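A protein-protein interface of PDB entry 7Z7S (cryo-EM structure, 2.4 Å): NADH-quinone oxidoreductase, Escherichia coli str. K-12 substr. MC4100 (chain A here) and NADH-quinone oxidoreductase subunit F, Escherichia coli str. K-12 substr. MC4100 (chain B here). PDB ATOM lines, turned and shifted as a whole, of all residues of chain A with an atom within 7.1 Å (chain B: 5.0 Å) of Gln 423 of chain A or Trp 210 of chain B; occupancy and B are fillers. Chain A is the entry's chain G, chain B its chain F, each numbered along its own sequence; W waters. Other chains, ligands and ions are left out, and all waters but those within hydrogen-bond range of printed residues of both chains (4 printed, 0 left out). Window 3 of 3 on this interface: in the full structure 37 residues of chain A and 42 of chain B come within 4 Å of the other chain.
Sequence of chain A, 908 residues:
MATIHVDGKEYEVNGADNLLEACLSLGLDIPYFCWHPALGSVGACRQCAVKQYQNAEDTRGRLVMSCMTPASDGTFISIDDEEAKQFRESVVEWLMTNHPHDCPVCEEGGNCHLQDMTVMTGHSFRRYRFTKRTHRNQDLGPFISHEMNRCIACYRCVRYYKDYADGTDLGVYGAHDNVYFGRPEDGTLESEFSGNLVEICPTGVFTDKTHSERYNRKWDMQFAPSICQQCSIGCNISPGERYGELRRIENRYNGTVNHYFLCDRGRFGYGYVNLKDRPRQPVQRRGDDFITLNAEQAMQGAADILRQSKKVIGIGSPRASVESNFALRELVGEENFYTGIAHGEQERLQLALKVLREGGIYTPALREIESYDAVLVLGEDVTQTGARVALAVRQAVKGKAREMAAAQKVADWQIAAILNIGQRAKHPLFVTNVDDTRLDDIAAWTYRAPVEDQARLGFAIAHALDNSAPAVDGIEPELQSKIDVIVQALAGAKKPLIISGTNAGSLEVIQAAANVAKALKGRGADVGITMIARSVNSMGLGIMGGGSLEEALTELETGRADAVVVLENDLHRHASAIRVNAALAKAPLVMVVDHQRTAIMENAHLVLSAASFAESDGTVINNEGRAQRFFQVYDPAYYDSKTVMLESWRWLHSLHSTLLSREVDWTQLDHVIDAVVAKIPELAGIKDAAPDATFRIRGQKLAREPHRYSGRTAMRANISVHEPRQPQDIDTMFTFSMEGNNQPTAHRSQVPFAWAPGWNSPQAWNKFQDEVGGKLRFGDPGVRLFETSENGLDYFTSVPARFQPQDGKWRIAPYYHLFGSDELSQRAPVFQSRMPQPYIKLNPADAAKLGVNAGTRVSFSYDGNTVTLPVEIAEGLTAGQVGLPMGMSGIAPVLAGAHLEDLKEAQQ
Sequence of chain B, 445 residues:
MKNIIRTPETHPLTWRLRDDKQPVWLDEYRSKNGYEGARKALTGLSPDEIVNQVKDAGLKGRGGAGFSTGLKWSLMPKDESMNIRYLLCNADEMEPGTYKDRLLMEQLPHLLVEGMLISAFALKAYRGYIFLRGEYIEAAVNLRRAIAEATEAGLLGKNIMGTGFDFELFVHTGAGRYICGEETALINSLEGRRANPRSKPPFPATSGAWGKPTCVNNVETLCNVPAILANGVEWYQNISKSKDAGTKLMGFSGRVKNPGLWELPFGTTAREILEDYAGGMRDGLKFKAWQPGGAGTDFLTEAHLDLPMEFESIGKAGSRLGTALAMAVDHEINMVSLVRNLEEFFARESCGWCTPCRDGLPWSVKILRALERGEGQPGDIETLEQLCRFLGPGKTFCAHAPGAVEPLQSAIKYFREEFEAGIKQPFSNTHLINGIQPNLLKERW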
ATOM      1  N   ALA A 401      30.447   1.926  18.672  1.00  0.00           N
ATOM      2  CA  ALA A 401      31.222   2.287  19.850  1.00  0.00           C
ATOM      3  C   ALA A 401      32.599   2.785  19.455  1.00  0.00           C
ATOM      4  O   ALA A 401      33.118   3.734  20.058  1.00  0.00           O
ATOM      5  CB  ALA A 401      31.340   1.092  20.792  1.00  0.00           C
ATOM      6  N   MET A 404      32.062   6.448  18.263  1.00  0.00           N
ATOM      7  CA  MET A 404      31.796   7.344  19.385  1.00  0.00           C
ATOM      8  C   MET A 404      33.056   7.607  20.193  1.00  0.00           C
ATOM      9  O   MET A 404      33.279   8.728  20.661  1.00  0.00           O
ATOM     10  CB  MET A 404      30.717   6.761  20.290  1.00  0.00           C
ATOM     11  CG  MET A 404      29.351   6.655  19.666  1.00  0.00           C
ATOM     12  SD  MET A 404      28.288   5.564  20.624  1.00  0.00           S
ATOM     13  CE  MET A 404      28.369   6.355  22.222  1.00  0.00           C
ATOM     14  N   ALA A 417      38.261   1.767  27.266  1.00  0.00           N
ATOM     15  CA  ALA A 417      37.623   3.075  27.186  1.00  0.00           C
ATOM     16  C   ALA A 417      36.616   3.137  26.043  1.00  0.00           C
ATOM     17  O   ALA A 417      35.562   3.768  26.174  1.00  0.00           O
ATOM     18  CB  ALA A 417      38.683   4.163  27.033  1.00  0.00           C
ATOM     19  N   ILE A 418      36.924   2.485  24.919  1.00  0.00           N
ATOM     20  CA  ILE A 418      36.000   2.437  23.785  1.00  0.00           C
ATOM     21  C   ILE A 418      34.721   1.707  24.171  1.00  0.00           C
ATOM     22  O   ILE A 418      33.610   2.162  23.877  1.00  0.00           O
ATOM     23  CB  ILE A 418      36.678   1.774  22.572  1.00  0.00           C
ATOM     24  CG1 ILE A 418      37.864   2.607  22.087  1.00  0.00           C
ATOM     25  CG2 ILE A 418      35.679   1.541  21.448  1.00  0.00           C
ATOM     26  CD1 ILE A 418      38.797   1.869  21.176  1.00  0.00           C
ATOM     27  N   LEU A 419      34.859   0.567  24.848  1.00  0.00           N
ATOM     28  CA  LEU A 419      33.690  -0.191  25.272  1.00  0.00           C
ATOM     29  C   LEU A 419      32.906   0.541  26.350  1.00  0.00           C
ATOM     30  O   LEU A 419      31.679   0.425  26.402  1.00  0.00           O
ATOM     31  CB  LEU A 419      34.106  -1.577  25.762  1.00  0.00           C
ATOM     32  CG  LEU A 419      34.726  -2.509  24.720  1.00  0.00           C
ATOM     33  CD1 LEU A 419      34.868  -3.921  25.267  1.00  0.00           C
ATOM     34  CD2 LEU A 419      33.926  -2.498  23.430  1.00  0.00           C
ATOM     35  N   ASN A 420      33.592   1.289  27.216  1.00  0.00           N
ATOM     36  CA  ASN A 420      32.897   2.077  28.225  1.00  0.00           C
ATOM     37  C   ASN A 420      32.100   3.212  27.597  1.00  0.00           C
ATOM     38  O   ASN A 420      30.982   3.503  28.033  1.00  0.00           O
ATOM     39  CB  ASN A 420      33.896   2.624  29.243  1.00  0.00           C
ATOM     40  CG  ASN A 420      33.238   3.484  30.293  1.00  0.00           C
ATOM     41  OD1 ASN A 420      32.313   3.051  30.970  1.00  0.00           O
ATOM     42  ND2 ASN A 420      33.704   4.715  30.428  1.00  0.00           N
ATOM     43  N   ILE A 421      32.657   3.867  26.577  1.00  0.00           N
ATOM     44  CA  ILE A 421      31.958   4.973  25.930  1.00  0.00           C
ATOM     45  C   ILE A 421      30.739   4.466  25.170  1.00  0.00           C
ATOM     46  O   ILE A 421      29.646   5.037  25.265  1.00  0.00           O
ATOM     47  CB  ILE A 421      32.923   5.748  25.014  1.00  0.00           C
ATOM     48  CG1 ILE A 421      33.820   6.654  25.848  1.00  0.00           C
ATOM     49  CG2 ILE A 421      32.174   6.571  23.984  1.00  0.00           C
ATOM     50  CD1 ILE A 421      35.042   7.108  25.129  1.00  0.00           C
ATOM     51  N   GLY A 422      30.902   3.377  24.422  1.00  0.00           N
ATOM     52  CA  GLY A 422      29.815   2.884  23.595  1.00  0.00           C
ATOM     53  C   GLY A 422      28.648   2.327  24.386  1.00  0.00           C
ATOM     54  O   GLY A 422      27.492   2.510  24.001  1.00  0.00           O
ATOM     55  N   GLN A 423      28.937   1.646  25.500  1.00  0.00           N
ATOM     56  CA  GLN A 423      27.954   0.985  26.368  1.00  0.00           C
ATOM     57  C   GLN A 423      27.200  -0.039  25.528  1.00  0.00           C
ATOM     58  O   GLN A 423      27.839  -0.971  25.014  1.00  0.00           O
ATOM     59  CB  GLN A 423      27.089   2.027  27.081  1.00  0.00           C
ATOM     60  CG  GLN A 423      27.762   2.662  28.264  1.00  0.00           C
ATOM     61  CD  GLN A 423      28.169   1.655  29.313  1.00  0.00           C
ATOM     62  OE1 GLN A 423      27.336   0.935  29.850  1.00  0.00           O
ATOM     63  NE2 GLN A 423      29.454   1.601  29.611  1.00  0.00           N
ATOM     64  N   ARG A 424      25.887   0.077  25.357  1.00  0.00           N
ATOM     65  CA  ARG A 424      25.126  -0.877  24.564  1.00  0.00           C
ATOM     66  C   ARG A 424      24.810  -0.366  23.164  1.00  0.00           C
ATOM     67  O   ARG A 424      24.037  -1.004  22.446  1.00  0.00           O
ATOM     68  CB  ARG A 424      23.834  -1.257  25.288  1.00  0.00           C
ATOM     69  CG  ARG A 424      24.010  -2.349  26.330  1.00  0.00           C
ATOM     70  CD  ARG A 424      22.968  -2.258  27.431  1.00  0.00           C
ATOM     71  NE  ARG A 424      22.745  -0.892  27.891  1.00  0.00           N
ATOM     72  CZ  ARG A 424      21.667  -0.491  28.551  1.00  0.00           C
ATOM     73  NH1 ARG A 424      20.685  -1.326  28.845  1.00  0.00           N
ATOM     74  NH2 ARG A 424      21.570   0.781  28.923  1.00  0.00           N
ATOM     75  N   ALA A 425      25.380   0.762  22.761  1.00  0.00           N
ATOM     76  CA  ALA A 425      25.137   1.283  21.424  1.00  0.00           C
ATOM     77  C   ALA A 425      25.854   0.441  20.377  1.00  0.00           C
ATOM     78  O   ALA A 425      27.003   0.036  20.565  1.00  0.00           O
ATOM     79  CB  ALA A 425      25.598   2.732  21.330  1.00  0.00           C
ATOM     80  N   LYS A 426      25.174   0.183  19.263  1.00  0.00           N
ATOM     81  CA  LYS A 426      25.784  -0.576  18.185  1.00  0.00           C
ATOM     82  C   LYS A 426      25.129  -0.231  16.860  1.00  0.00           C
ATOM     83  O   LYS A 426      24.023   0.310  16.808  1.00  0.00           O
ATOM     84  CB  LYS A 426      25.707  -2.083  18.446  1.00  0.00           C
ATOM     85  CG  LYS A 426      24.373  -2.597  18.905  1.00  0.00           C
ATOM     86  CD  LYS A 426      24.513  -4.014  19.428  1.00  0.00           C
ATOM     87  CE  LYS A 426      23.321  -4.410  20.270  1.00  0.00           C
ATOM     88  NZ  LYS A 426      23.163  -3.515  21.452  1.00  0.00           N
ATOM     89  N   TYR B  86      26.520  12.321  36.291  1.00  0.00           N
ATOM     90  CA  TYR B  86      26.481  11.560  37.527  1.00  0.00           C
ATOM     91  C   TYR B  86      27.447  12.122  38.556  1.00  0.00           C
ATOM     92  O   TYR B  86      28.590  12.472  38.240  1.00  0.00           O
ATOM     93  CB  TYR B  86      26.796  10.097  37.269  1.00  0.00           C
ATOM     94  CG  TYR B  86      25.736   9.419  36.456  1.00  0.00           C
ATOM     95  CD1 TYR B  86      24.512   9.101  37.015  1.00  0.00           C
ATOM     96  CD2 TYR B  86      25.952   9.104  35.124  1.00  0.00           C
ATOM     97  CE1 TYR B  86      23.538   8.487  36.277  1.00  0.00           C
ATOM     98  CE2 TYR B  86      24.979   8.490  34.378  1.00  0.00           C
ATOM     99  CZ  TYR B  86      23.774   8.185  34.961  1.00  0.00           C
ATOM    100  OH  TYR B  86      22.798   7.570  34.223  1.00  0.00           O
ATOM    101  N   TYR B 129      24.684   9.063  43.339  1.00  0.00           N
ATOM    102  CA  TYR B 129      24.727   7.785  44.035  1.00  0.00           C
ATOM    103  C   TYR B 129      25.719   7.875  45.178  1.00  0.00           C
ATOM    104  O   TYR B 129      26.832   8.368  44.994  1.00  0.00           O
ATOM    105  CB  TYR B 129      25.126   6.645  43.098  1.00  0.00           C
ATOM    106  CG  TYR B 129      24.139   6.368  41.995  1.00  0.00           C
ATOM    107  CD1 TYR B 129      23.070   5.514  42.195  1.00  0.00           C
ATOM    108  CD2 TYR B 129      24.282   6.958  40.751  1.00  0.00           C
ATOM    109  CE1 TYR B 129      22.170   5.260  41.190  1.00  0.00           C
ATOM    110  CE2 TYR B 129      23.389   6.710  39.745  1.00  0.00           C
ATOM    111  CZ  TYR B 129      22.337   5.862  39.967  1.00  0.00           C
ATOM    112  OH  TYR B 129      21.444   5.614  38.959  1.00  0.00           O
ATOM    113  N   LEU B 190      29.622   0.152  40.631  1.00  0.00           N
ATOM    114  CA  LEU B 190      28.307   0.767  40.505  1.00  0.00           C
ATOM    115  C   LEU B 190      27.574   0.270  39.269  1.00  0.00           C
ATOM    116  O   LEU B 190      26.351   0.119  39.297  1.00  0.00           O
ATOM    117  CB  LEU B 190      28.444   2.287  40.470  1.00  0.00           C
ATOM    118  CG  LEU B 190      27.147   3.081  40.323  1.00  0.00           C
ATOM    119  CD1 LEU B 190      26.421   3.170  41.645  1.00  0.00           C
ATOM    120  CD2 LEU B 190      27.430   4.452  39.758  1.00  0.00           C
ATOM    121  N   GLU B 191      28.303  -0.030  38.198  1.00  0.00           N
ATOM    122  CA  GLU B 191      27.722  -0.592  36.987  1.00  0.00           C
ATOM    123  C   GLU B 191      27.394  -2.072  37.113  1.00  0.00           C
ATOM    124  O   GLU B 191      26.934  -2.669  36.138  1.00  0.00           O
ATOM    125  CB  GLU B 191      28.666  -0.378  35.805  1.00  0.00           C
ATOM    126  CG  GLU B 191      28.814   1.066  35.384  1.00  0.00           C
ATOM    127  CD  GLU B 191      29.706   1.228  34.176  1.00  0.00           C
ATOM    128  OE1 GLU B 191      29.920   0.237  33.455  1.00  0.00           O
ATOM    129  OE2 GLU B 191      30.201   2.343  33.946  1.00  0.00           O
ATOM    130  N   ARG B 193      29.570  -4.612  37.819  1.00  0.00           N
ATOM    131  CA  ARG B 193      30.649  -5.447  37.322  1.00  0.00           C
ATOM    132  C   ARG B 193      31.642  -5.735  38.436  1.00  0.00           C
ATOM    133  O   ARG B 193      31.539  -5.211  39.547  1.00  0.00           O
ATOM    134  CB  ARG B 193      31.354  -4.773  36.145  1.00  0.00           C
ATOM    135  CG  ARG B 193      30.424  -4.048  35.213  1.00  0.00           C
ATOM    136  CD  ARG B 193      31.191  -3.283  34.167  1.00  0.00           C
ATOM    137  NE  ARG B 193      30.332  -2.855  33.071  1.00  0.00           N
ATOM    138  CZ  ARG B 193      29.995  -3.616  32.040  1.00  0.00           C
ATOM    139  NH1 ARG B 193      30.427  -4.860  31.928  1.00  0.00           N
ATOM    140  NH2 ARG B 193      29.200  -3.118  31.100  1.00  0.00           N
ATOM    141  N   GLY B 208      32.757   8.376  32.451  1.00  0.00           N
ATOM    142  CA  GLY B 208      32.812   7.604  33.672  1.00  0.00           C
ATOM    143  C   GLY B 208      31.735   6.552  33.772  1.00  0.00           C
ATOM    144  O   GLY B 208      31.793   5.531  33.086  1.00  0.00           O
ATOM    145  N   ALA B 209      30.747   6.795  34.624  1.00  0.00           N
ATOM    146  CA  ALA B 209      29.688   5.825  34.867  1.00  0.00           C
ATOM    147  C   ALA B 209      28.782   5.720  33.652  1.00  0.00           C
ATOM    148  O   ALA B 209      28.147   6.702  33.259  1.00  0.00           O
ATOM    149  CB  ALA B 209      28.890   6.220  36.104  1.00  0.00           C
ATOM    150  N   TRP B 210      28.737   4.522  33.061  1.00  0.00           N
ATOM    151  CA  TRP B 210      27.986   4.225  31.838  1.00  0.00           C
ATOM    152  C   TRP B 210      28.391   5.137  30.686  1.00  0.00           C
ATOM    153  O   TRP B 210      27.565   5.498  29.848  1.00  0.00           O
ATOM    154  CB  TRP B 210      26.474   4.289  32.076  1.00  0.00           C
ATOM    155  CG  TRP B 210      26.011   3.394  33.177  1.00  0.00           C
ATOM    156  CD1 TRP B 210      25.840   2.048  33.116  1.00  0.00           C
ATOM    157  CD2 TRP B 210      25.669   3.782  34.509  1.00  0.00           C
ATOM    158  NE1 TRP B 210      25.410   1.570  34.324  1.00  0.00           N
ATOM    159  CE2 TRP B 210      25.296   2.616  35.198  1.00  0.00           C
ATOM    160  CE3 TRP B 210      25.637   5.001  35.186  1.00  0.00           C
ATOM    161  CZ2 TRP B 210      24.900   2.632  36.529  1.00  0.00           C
ATOM    162  CZ3 TRP B 210      25.246   5.015  36.506  1.00  0.00           C
ATOM    163  CH2 TRP B 210      24.882   3.839  37.164  1.00  0.00           C
ATOM    164  N   GLY B 211      29.664   5.525  30.644  1.00  0.00           N
ATOM    165  CA  GLY B 211      30.185   6.380  29.604  1.00  0.00           C
ATOM    166  C   GLY B 211      29.880   7.851  29.760  1.00  0.00           C
ATOM    167  O   GLY B 211      30.404   8.658  28.984  1.00  0.00           O
ATOM    168  N   LYS B 212      29.065   8.228  30.724  1.00  0.00           N
ATOM    169  CA  LYS B 212      28.651   9.604  30.928  1.00  0.00           C
ATOM    170  C   LYS B 212      29.677  10.353  31.757  1.00  0.00           C
ATOM    171  O   LYS B 212      30.508   9.742  32.430  1.00  0.00           O
ATOM    172  CB  LYS B 212      27.293   9.644  31.618  1.00  0.00           C
ATOM    173  CG  LYS B 212      26.237   8.823  30.929  1.00  0.00           C
ATOM    174  CD  LYS B 212      25.992   9.324  29.528  1.00  0.00           C
ATOM    175  CE  LYS B 212      25.361   8.253  28.670  1.00  0.00           C
ATOM    176  NZ  LYS B 212      24.204   7.609  29.337  1.00  0.00           N
HETATM  177  O   HOH W   1      27.684  -0.599  31.764  1.00  0.00           O
HETATM  178  O   HOH W   2      27.799  -2.024  28.287  1.00  0.00           O
HETATM  179  O   HOH W   3      28.946   7.428  26.195  1.00  0.00           O
HETATM  180  O   HOH W   4      31.642   0.217  31.201  1.00  0.00           O
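Among the printed residues, pairs that only touch across the chains: Gln 423 of chain A with Trp 210 of chain B, Asn 420 of chain A with Gly 211 of chain B and Asn 420 of chain A with Glu 191 of chain B.
Of chain B, only Trp 210 comes within 4 Å of Gln 423 of chain A.
Trp 210 of chain B touches one residue of chain A.
Of the printed residues of chain A, Gly 208 of chain B touches Asn 420.
Printed residues of chain A within 4 Å of Glu 191 of chain B: Asn 420.
Of the printed residues of chain A, Gly 211 of chain B touches Asn 420.
Of the printed residues of chain B, Asn 420 of chain A touches Glu 191 (3.7 Å), Gly 208 (3.3 Å) and Gly 211 (3.4 Å).
Tyr 129 of chain B touches none of the printed residues of chain A.
The nearest residue of chain A that does not touch Trp 210 of chain B is Asn 420 of chain A (4.1 Å).
The nearest printed residue of chain A that does not touch Glu 191 of chain B is Gln 423 of chain A (4.1 Å).
Of the 12 printed residues of chain A, 2 touch a printed residue of chain B.
Printed residues of chain B that touch a printed residue of chain A: Glu 191, Gly 208, Trp 210 and Gly 211.
The backbone carbonyl oxygen of Gly 208 of chain B lies close to the side-chain amide oxygen of Asn 420 of chain A.
Water W1 lies within hydrogen-bond range of OE1 of Gln 423 of chain A, OE1 of Glu 191 of chain B and NH2 of Arg 193 of chain B.
Water W3 lies within hydrogen-bond range of the backbone carbonyl oxygen of Ile 421 of chain A and the backbone carbonyl oxygen of Gly 211 of chain B.
Water W4 lies within hydrogen-bond range of OE1 of Glu 191 of chain B (2.8 Å), OD1 of Asn 420 of chain A (2.9 Å) and NE2 of Gln 423 of chain A (3.0 Å).
Water W2 lies within hydrogen-bond range of NH2 of Arg 193 of chain B and OE1 of Gln 423 of chain A.
The side-chain carboxylate (OE1) of Glu 191 of chain B lies within salt-bridge range of the guanidinium group (NE) of Arg 193 of chain B.
The backbone carbonyl oxygen (O) of Asn 420 of chain A lies within hydrogen-bond range of the side-chain amide nitrogen (NE2) of Gln 423 of chain A (2.9 Å).
OE2 of Glu 191 of chain B sits at hydrogen-bond distance from N of Trp 210 of chain B (2.8 Å).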
